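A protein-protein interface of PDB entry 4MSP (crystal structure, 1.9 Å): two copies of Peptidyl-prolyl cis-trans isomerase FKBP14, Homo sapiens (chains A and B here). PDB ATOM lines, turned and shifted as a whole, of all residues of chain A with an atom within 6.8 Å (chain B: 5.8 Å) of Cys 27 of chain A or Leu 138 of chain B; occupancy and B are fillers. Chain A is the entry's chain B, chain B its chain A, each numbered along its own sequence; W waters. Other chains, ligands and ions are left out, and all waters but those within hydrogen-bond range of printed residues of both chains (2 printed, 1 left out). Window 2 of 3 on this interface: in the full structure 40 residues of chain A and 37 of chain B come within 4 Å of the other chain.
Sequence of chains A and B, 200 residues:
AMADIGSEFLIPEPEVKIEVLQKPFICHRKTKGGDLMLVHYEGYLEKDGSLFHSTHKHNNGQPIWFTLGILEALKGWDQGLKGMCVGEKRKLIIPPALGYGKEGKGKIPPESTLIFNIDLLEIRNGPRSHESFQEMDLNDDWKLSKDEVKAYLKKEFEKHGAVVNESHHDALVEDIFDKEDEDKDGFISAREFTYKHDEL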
ATOM      1  N   LYS A  23       9.279 -17.816  17.373  1.00  0.00           N
ATOM      2  CA  LYS A  23       8.299 -18.552  18.167  1.00  0.00           C
ATOM      3  C   LYS A  23       8.702 -18.502  19.648  1.00  0.00           C
ATOM      4  O   LYS A  23       9.870 -18.331  19.970  1.00  0.00           O
ATOM      5  CB  LYS A  23       8.239 -20.019  17.717  1.00  0.00           C
ATOM      6  CG  LYS A  23       7.422 -20.300  16.469  1.00  0.00           C
ATOM      7  CD  LYS A  23       5.931 -20.419  16.771  1.00  0.00           C
ATOM      8  CE  LYS A  23       5.164 -20.921  15.544  1.00  0.00           C
ATOM      9  NZ  LYS A  23       3.691 -21.068  15.792  1.00  0.00           N
ATOM     10  N   PRO A  24       7.729 -18.671  20.557  1.00  0.00           N
ATOM     11  CA  PRO A  24       8.070 -18.739  21.980  1.00  0.00           C
ATOM     12  C   PRO A  24       8.821 -20.030  22.266  1.00  0.00           C
ATOM     13  O   PRO A  24       8.758 -20.956  21.447  1.00  0.00           O
ATOM     14  CB  PRO A  24       6.697 -18.766  22.653  1.00  0.00           C
ATOM     15  CG  PRO A  24       5.790 -19.393  21.633  1.00  0.00           C
ATOM     16  CD  PRO A  24       6.280 -18.807  20.332  1.00  0.00           C
ATOM     17  N   PHE A  25       9.528 -20.091  23.391  1.00  0.00           N
ATOM     18  CA  PHE A  25      10.185 -21.322  23.810  1.00  0.00           C
ATOM     19  C   PHE A  25       9.144 -22.431  23.904  1.00  0.00           C
ATOM     20  O   PHE A  25       9.400 -23.578  23.524  1.00  0.00           O
ATOM     21  CB  PHE A  25      10.877 -21.128  25.166  1.00  0.00           C
ATOM     22  CG  PHE A  25      11.715 -22.305  25.607  1.00  0.00           C
ATOM     23  CD1 PHE A  25      12.168 -23.245  24.691  1.00  0.00           C
ATOM     24  CD2 PHE A  25      12.049 -22.468  26.942  1.00  0.00           C
ATOM     25  CE1 PHE A  25      12.939 -24.327  25.103  1.00  0.00           C
ATOM     26  CE2 PHE A  25      12.818 -23.546  27.357  1.00  0.00           C
ATOM     27  CZ  PHE A  25      13.263 -24.474  26.434  1.00  0.00           C
ATOM     28  N   ILE A  26       7.963 -22.083  24.409  1.00  0.00           N
ATOM     29  CA  ILE A  26       6.896 -23.052  24.573  1.00  0.00           C
ATOM     30  C   ILE A  26       5.562 -22.444  24.193  1.00  0.00           C
ATOM     31  O   ILE A  26       5.215 -21.348  24.638  1.00  0.00           O
ATOM     32  CB  ILE A  26       6.793 -23.546  26.022  1.00  0.00           C
ATOM     33  CG1 ILE A  26       8.115 -24.152  26.494  1.00  0.00           C
ATOM     34  CG2 ILE A  26       5.683 -24.568  26.144  1.00  0.00           C
ATOM     35  CD1 ILE A  26       8.056 -24.683  27.925  1.00  0.00           C
ATOM     36  N   CYS A  27       4.821 -23.144  23.340  1.00  0.00           N
ATOM     37  CA  CYS A  27       3.502 -22.676  22.929  1.00  0.00           C
ATOM     38  C   CYS A  27       2.409 -23.469  23.637  1.00  0.00           C
ATOM     39  O   CYS A  27       2.367 -24.697  23.543  1.00  0.00           O
ATOM     40  CB  CYS A  27       3.324 -22.806  21.420  1.00  0.00           C
ATOM     41  SG  CYS A  27       1.719 -22.180  20.856  1.00  0.00           S
ATOM     42  N   HIS A  28       1.524 -22.767  24.340  1.00  0.00           N
ATOM     43  CA  HIS A  28       0.482 -23.423  25.114  1.00  0.00           C
ATOM     44  C   HIS A  28      -0.882 -23.342  24.447  1.00  0.00           C
ATOM     45  O   HIS A  28      -1.832 -24.000  24.891  1.00  0.00           O
ATOM     46  CB  HIS A  28       0.393 -22.818  26.518  1.00  0.00           C
ATOM     47  CG  HIS A  28       1.616 -23.046  27.346  1.00  0.00           C
ATOM     48  ND1 HIS A  28       2.000 -24.298  27.772  1.00  0.00           N
ATOM     49  CD2 HIS A  28       2.542 -22.183  27.828  1.00  0.00           C
ATOM     50  CE1 HIS A  28       3.111 -24.199  28.480  1.00  0.00           C
ATOM     51  NE2 HIS A  28       3.460 -22.927  28.529  1.00  0.00           N
ATOM     52  N   ARG A  29      -0.978 -22.544  23.388  1.00  0.00           N
ATOM     53  CA  ARG A  29      -2.263 -22.279  22.752  1.00  0.00           C
ATOM     54  C   ARG A  29      -2.066 -21.532  21.433  1.00  0.00           C
ATOM     55  O   ARG A  29      -1.256 -20.606  21.354  1.00  0.00           O
ATOM     56  CB  ARG A  29      -3.123 -21.436  23.690  1.00  0.00           C
ATOM     57  CG  ARG A  29      -4.416 -20.962  23.090  1.00  0.00           C
ATOM     58  CD  ARG A  29      -5.205 -20.140  24.096  1.00  0.00           C
ATOM     59  NE  ARG A  29      -6.530 -19.813  23.579  1.00  0.00           N
ATOM     60  CZ  ARG A  29      -7.418 -19.054  24.217  1.00  0.00           C
ATOM     61  NH1 ARG A  29      -7.124 -18.531  25.401  1.00  0.00           N
ATOM     62  NH2 ARG A  29      -8.601 -18.818  23.668  1.00  0.00           N
ATOM     63  N   LYS A  30      -2.803 -21.934  20.400  1.00  0.00           N
ATOM     64  CA  LYS A  30      -2.700 -21.297  19.083  1.00  0.00           C
ATOM     65  C   LYS A  30      -4.026 -20.646  18.687  1.00  0.00           C
ATOM     66  O   LYS A  30      -5.105 -21.161  18.998  1.00  0.00           O
ATOM     67  CB  LYS A  30      -2.294 -22.316  18.009  1.00  0.00           C
ATOM     68  CG  LYS A  30      -0.785 -22.630  17.936  1.00  0.00           C
ATOM     69  CD  LYS A  30      -0.510 -23.603  16.786  1.00  0.00           C
ATOM     70  CE  LYS A  30       0.993 -23.806  16.554  1.00  0.00           C
ATOM     71  NZ  LYS A  30       1.254 -24.596  15.310  1.00  0.00           N
ATOM     72  N   GLY A  83      -3.314 -19.991  13.963  1.00  0.00           N
ATOM     73  CA  GLY A  83      -2.346 -20.931  14.488  1.00  0.00           C
ATOM     74  C   GLY A  83      -1.124 -20.247  15.059  1.00  0.00           C
ATOM     75  O   GLY A  83      -0.008 -20.779  14.990  1.00  0.00           O
ATOM     76  N   MET A  84      -1.339 -19.066  15.620  1.00  0.00           N
ATOM     77  CA  MET A  84      -0.253 -18.241  16.130  1.00  0.00           C
ATOM     78  C   MET A  84      -0.196 -18.335  17.649  1.00  0.00           C
ATOM     79  O   MET A  84      -1.234 -18.447  18.289  1.00  0.00           O
ATOM     80  CB  MET A  84      -0.504 -16.791  15.738  1.00  0.00           C
ATOM     81  CG  MET A  84       0.708 -15.878  15.890  1.00  0.00           C
ATOM     82  SD  MET A  84       0.309 -14.281  15.164  1.00  0.00           S
ATOM     83  CE  MET A  84       1.878 -13.440  15.337  1.00  0.00           C
ATOM     84  N   CYS A  85       1.008 -18.256  18.221  1.00  0.00           N
ATOM     85  CA  CYS A  85       1.176 -18.409  19.666  1.00  0.00           C
ATOM     86  C   CYS A  85       1.539 -17.073  20.298  1.00  0.00           C
ATOM     87  O   CYS A  85       2.157 -16.242  19.651  1.00  0.00           O
ATOM     88  CB  CYS A  85       2.307 -19.403  19.985  1.00  0.00           C
ATOM     89  SG  CYS A  85       2.193 -21.058  19.221  1.00  0.00           S
ATOM     90  N   VAL A  86       1.212 -16.877  21.573  1.00  0.00           N
ATOM     91  CA  VAL A  86       1.766 -15.725  22.291  1.00  0.00           C
ATOM     92  C   VAL A  86       3.302 -15.733  22.271  1.00  0.00           C
ATOM     93  O   VAL A  86       3.947 -16.749  22.577  1.00  0.00           O
ATOM     94  CB  VAL A  86       1.283 -15.674  23.758  1.00  0.00           C
ATOM     95  CG1 VAL A  86       2.010 -14.588  24.515  1.00  0.00           C
ATOM     96  CG2 VAL A  86      -0.213 -15.444  23.795  1.00  0.00           C
ATOM     97  N   GLU A  88       4.901 -15.124  19.578  1.00  0.00           N
ATOM     98  CA  GLU A  88       5.242 -15.347  18.181  1.00  0.00           C
ATOM     99  C   GLU A  88       5.190 -14.031  17.416  1.00  0.00           C
ATOM    100  O   GLU A  88       4.387 -13.160  17.731  1.00  0.00           O
ATOM    101  CB  GLU A  88       4.293 -16.373  17.548  1.00  0.00           C
ATOM    102  CG  GLU A  88       4.502 -16.601  16.046  1.00  0.00           C
ATOM    103  CD  GLU A  88       3.644 -17.725  15.502  1.00  0.00           C
ATOM    104  OE1 GLU A  88       3.123 -18.520  16.314  1.00  0.00           O
ATOM    105  OE2 GLU A  88       3.500 -17.822  14.259  1.00  0.00           O
ATOM    106  N   PHE B 133      -5.222 -29.265  12.157  1.00  0.00           N
ATOM    107  CA  PHE B 133      -4.028 -29.978  12.602  1.00  0.00           C
ATOM    108  C   PHE B 133      -2.978 -29.002  13.129  1.00  0.00           C
ATOM    109  O   PHE B 133      -2.422 -29.192  14.212  1.00  0.00           O
ATOM    110  CB  PHE B 133      -3.449 -30.818  11.463  1.00  0.00           C
ATOM    111  CG  PHE B 133      -2.247 -31.639  11.859  1.00  0.00           C
ATOM    112  CD1 PHE B 133      -2.405 -32.912  12.386  1.00  0.00           C
ATOM    113  CD2 PHE B 133      -0.969 -31.142  11.705  1.00  0.00           C
ATOM    114  CE1 PHE B 133      -1.312 -33.665  12.751  1.00  0.00           C
ATOM    115  CE2 PHE B 133       0.130 -31.892  12.069  1.00  0.00           C
ATOM    116  CZ  PHE B 133      -0.043 -33.157  12.590  1.00  0.00           C
ATOM    117  N   GLN B 134      -2.712 -27.954  12.358  1.00  0.00           N
ATOM    118  CA  GLN B 134      -1.721 -26.966  12.754  1.00  0.00           C
ATOM    119  C   GLN B 134      -2.117 -26.279  14.057  1.00  0.00           C
ATOM    120  O   GLN B 134      -1.268 -26.013  14.901  1.00  0.00           O
ATOM    121  CB  GLN B 134      -1.518 -25.938  11.644  1.00  0.00           C
ATOM    122  CG  GLN B 134      -0.847 -26.528  10.405  1.00  0.00           C
ATOM    123  CD  GLN B 134      -0.576 -25.481   9.344  1.00  0.00           C
ATOM    124  OE1 GLN B 134      -1.296 -24.488   9.240  1.00  0.00           O
ATOM    125  NE2 GLN B 134       0.476 -25.686   8.568  1.00  0.00           N
ATOM    126  N   GLU B 135      -3.410 -26.016  14.222  1.00  0.00           N
ATOM    127  CA  GLU B 135      -3.906 -25.353  15.426  1.00  0.00           C
ATOM    128  C   GLU B 135      -3.654 -26.206  16.668  1.00  0.00           C
ATOM    129  O   GLU B 135      -3.354 -25.692  17.751  1.00  0.00           O
ATOM    130  CB  GLU B 135      -5.403 -25.073  15.293  1.00  0.00           C
ATOM    131  CG  GLU B 135      -5.987 -24.393  16.506  1.00  0.00           C
ATOM    132  CD  GLU B 135      -7.486 -24.527  16.577  1.00  0.00           C
ATOM    133  OE1 GLU B 135      -8.110 -24.818  15.529  1.00  0.00           O
ATOM    134  OE2 GLU B 135      -8.031 -24.352  17.688  1.00  0.00           O
ATOM    135  N   MET B 136      -3.766 -27.515  16.495  1.00  0.00           N
ATOM    136  CA  MET B 136      -3.548 -28.460  17.588  1.00  0.00           C
ATOM    137  C   MET B 136      -2.079 -28.747  17.823  1.00  0.00           C
ATOM    138  O   MET B 136      -1.657 -28.975  18.958  1.00  0.00           O
ATOM    139  CB  MET B 136      -4.295 -29.769  17.321  1.00  0.00           C
ATOM    140  CG  MET B 136      -5.817 -29.627  17.368  1.00  0.00           C
ATOM    141  SD  MET B 136      -6.660 -31.150  16.890  1.00  0.00           S
ATOM    142  CE  MET B 136      -6.511 -32.083  18.403  1.00  0.00           C
ATOM    143  N   ASP B 137      -1.303 -28.739  16.746  1.00  0.00           N
ATOM    144  CA  ASP B 137       0.119 -29.055  16.821  1.00  0.00           C
ATOM    145  C   ASP B 137       0.901 -27.882  17.410  1.00  0.00           C
ATOM    146  O   ASP B 137       1.579 -27.150  16.678  1.00  0.00           O
ATOM    147  CB  ASP B 137       0.652 -29.403  15.426  1.00  0.00           C
ATOM    148  CG  ASP B 137       2.109 -29.773  15.441  1.00  0.00           C
ATOM    149  OD1 ASP B 137       2.606 -30.131  16.529  1.00  0.00           O
ATOM    150  OD2 ASP B 137       2.762 -29.711  14.375  1.00  0.00           O
ATOM    151  N   LEU B 138       0.807 -27.715  18.731  1.00  0.00           N
ATOM    152  CA  LEU B 138       1.367 -26.547  19.408  1.00  0.00           C
ATOM    153  C   LEU B 138       2.872 -26.365  19.196  1.00  0.00           C
ATOM    154  O   LEU B 138       3.350 -25.235  19.109  1.00  0.00           O
ATOM    155  CB  LEU B 138       1.050 -26.576  20.910  1.00  0.00           C
ATOM    156  CG  LEU B 138      -0.438 -26.557  21.307  1.00  0.00           C
ATOM    157  CD1 LEU B 138      -0.609 -26.658  22.819  1.00  0.00           C
ATOM    158  CD2 LEU B 138      -1.137 -25.322  20.776  1.00  0.00           C
ATOM    159  N   ASN B 139       3.622 -27.459  19.107  1.00  0.00           N
ATOM    160  CA  ASN B 139       5.076 -27.335  18.987  1.00  0.00           C
ATOM    161  C   ASN B 139       5.624 -27.519  17.570  1.00  0.00           C
ATOM    162  O   ASN B 139       6.833 -27.694  17.382  1.00  0.00           O
ATOM    163  CB  ASN B 139       5.792 -28.274  19.962  1.00  0.00           C
ATOM    164  CG  ASN B 139       5.716 -29.727  19.541  1.00  0.00           C
ATOM    165  OD1 ASN B 139       4.886 -30.106  18.711  1.00  0.00           O
ATOM    166  ND2 ASN B 139       6.576 -30.556  20.126  1.00  0.00           N
ATOM    167  N   ASP B 140       4.730 -27.491  16.585  1.00  0.00           N
ATOM    168  CA  ASP B 140       5.114 -27.554  15.169  1.00  0.00           C
ATOM    169  C   ASP B 140       6.031 -28.726  14.793  1.00  0.00           C
ATOM    170  O   ASP B 140       6.878 -28.588  13.902  1.00  0.00           O
ATOM    171  CB  ASP B 140       5.774 -26.238  14.737  1.00  0.00           C
ATOM    172  CG  ASP B 140       4.938 -25.017  15.081  1.00  0.00           C
ATOM    173  OD1 ASP B 140       3.743 -24.981  14.731  1.00  0.00           O
ATOM    174  OD2 ASP B 140       5.482 -24.094  15.714  1.00  0.00           O
ATOM    175  N   LEU B 144       0.741 -34.789  16.770  1.00  0.00           N
ATOM    176  CA  LEU B 144      -0.034 -34.345  17.923  1.00  0.00           C
ATOM    177  C   LEU B 144       0.247 -35.253  19.105  1.00  0.00           C
ATOM    178  O   LEU B 144      -0.014 -36.452  19.030  1.00  0.00           O
ATOM    179  CB  LEU B 144      -1.521 -34.393  17.597  1.00  0.00           C
ATOM    180  CG  LEU B 144      -1.918 -33.742  16.274  1.00  0.00           C
ATOM    181  CD1 LEU B 144      -3.425 -33.808  16.085  1.00  0.00           C
ATOM    182  CD2 LEU B 144      -1.430 -32.312  16.234  1.00  0.00           C
ATOM    183  N   ASP B 147      -0.801 -34.614  25.058  1.00  0.00           N
ATOM    184  CA  ASP B 147      -0.966 -33.353  25.777  1.00  0.00           C
ATOM    185  C   ASP B 147      -1.560 -32.276  24.873  1.00  0.00           C
ATOM    186  O   ASP B 147      -2.377 -31.457  25.310  1.00  0.00           O
ATOM    187  CB  ASP B 147       0.365 -32.874  26.370  1.00  0.00           C
ATOM    188  CG  ASP B 147       0.695 -33.540  27.697  1.00  0.00           C
ATOM    189  OD1 ASP B 147      -0.138 -34.304  28.234  1.00  0.00           O
ATOM    190  OD2 ASP B 147       1.793 -33.275  28.215  1.00  0.00           O
ATOM    191  N   GLU B 148      -1.162 -32.281  23.605  1.00  0.00           N
ATOM    192  CA  GLU B 148      -1.719 -31.309  22.655  1.00  0.00           C
ATOM    193  C   GLU B 148      -3.205 -31.567  22.409  1.00  0.00           C
ATOM    194  O   GLU B 148      -4.014 -30.630  22.355  1.00  0.00           O
ATOM    195  CB  GLU B 148      -0.923 -31.323  21.344  1.00  0.00           C
ATOM    196  CG  GLU B 148       0.446 -30.669  21.479  1.00  0.00           C
ATOM    197  CD  GLU B 148       1.348 -30.935  20.293  1.00  0.00           C
ATOM    198  OE1 GLU B 148       1.013 -31.836  19.499  1.00  0.00           O
ATOM    199  OE2 GLU B 148       2.387 -30.247  20.159  1.00  0.00           O
ATOM    200  N   ALA B 151      -5.060 -30.491  25.446  1.00  0.00           N
ATOM    201  CA  ALA B 151      -5.184 -29.035  25.497  1.00  0.00           C
ATOM    202  C   ALA B 151      -6.335 -28.560  24.623  1.00  0.00           C
ATOM    203  O   ALA B 151      -7.100 -27.666  24.998  1.00  0.00           O
ATOM    204  CB  ALA B 151      -3.879 -28.360  25.070  1.00  0.00           C
HETATM  205  O   HOH W   1       2.787 -22.420  13.300  1.00  0.00           O
HETATM  206  O   HOH W   2      -4.589 -24.342  20.159  1.00  0.00           O
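The side-chain carboxylate of Asp 140 of chain B lies within salt-bridge range of the side-chain amino group of Lys 23 of chain A (3.5 Å).
NZ of Lys 30 of chain A lies within salt-bridge range of OD1 of Asp 140 of chain B, 2.6 Å away.
NZ of Lys 30 of chain A sits at hydrogen-bond distance from O of Asp 137 of chain B, 2.9 Å away.
O of Gln 134 of chain B sits at hydrogen-bond distance from NZ of Lys 30 of chain A.
N of Arg 29 of chain A sits close to SG of Cys 27 of chain A, at 3.7 Å.
SG of Cys 85 of chain A forms a disulfide with SG of Cys 27 of chain A (2.0 Å).
SG of Cys 85 of chain A is in hydrogen-bond range of NZ of Lys 23 of chain A (3.7 Å).
The side-chain carboxylate (OE2) of Glu 148 of chain B lies close to the backbone NH (N) of Leu 138 of chain B.
The side-chain amino group of Lys 23 of chain A lies within salt-bridge range of the side-chain carboxylate of Glu 88 of chain A.
OD1 of Asp 137 of chain B sits close to N of Asp 140 of chain B, at 3.4 Å.
Among the printed residues, pairs that only touch across the chains: Cys 27 of chain A with Leu 138 of chain B (3.4 Å), Lys 30 of chain A with Glu 135 of chain B (3.5 Å), His 28 of chain A with Leu 138 of chain B (3.6 Å), Lys 30 of chain A with Leu 138 of chain B (3.8 Å) and Arg 29 of chain A with Leu 138 of chain B (3.8 Å).
Cys 27 of chain A touches just one residue of chain B: Leu 138 (3.4 Å).
Leu 138 of chain B touches just these residues of chain A: Cys 27, His 28, Arg 29 and Lys 30.
Of the printed residues of chain B, Lys 23 of chain A touches Asp 140 (3.2 Å).
Of the printed residues of chain A, Gln 134 of chain B touches Lys 30 (2.9 Å).
Printed residues of chain B within 4 Å of His 28 of chain A: Leu 138 (3.6 Å).
Ala 151 of chain B touches none of the printed residues of chain A.
The nearest residue of chain B that does not touch Cys 27 of chain A is Asn 139 of chain B (5.2 Å).
Printed residues of chain A that touch a printed residue of chain B: Lys 23, Cys 27, His 28, Arg 29 and Lys 30.
Along chain A the printed residues that touch a printed residue of chain B span positions 23 to 30.
Of the 12 printed residues of chain B, 5 touch a printed residue of chain A.
Among the printed residues, 9 pairs touch across the chains.
Among the printed residues, Asp or Glu carboxylates within 4 Å of a Lys or Arg side-chain nitrogen of the other chain: Lys 23 of chain A with Asp 140 of chain B (3.5 Å) and Lys 30 of chain A with Asp 140 of chain B (2.6 Å).
No position is printed for both chains.
Of the 9 pairs that touch across the chains among the printed residues, none has its exchanged pair printed and touching as well.
Water W1 lies within hydrogen-bond range of NZ of Lys 23 of chain A (3.0 Å), OD1 of Asp 140 of chain B (3.1 Å) and NZ of Lys 30 of chain A (3.3 Å).
Water W2 bridges N of Lys 30 of chain A and O of Glu 135 of chain B.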
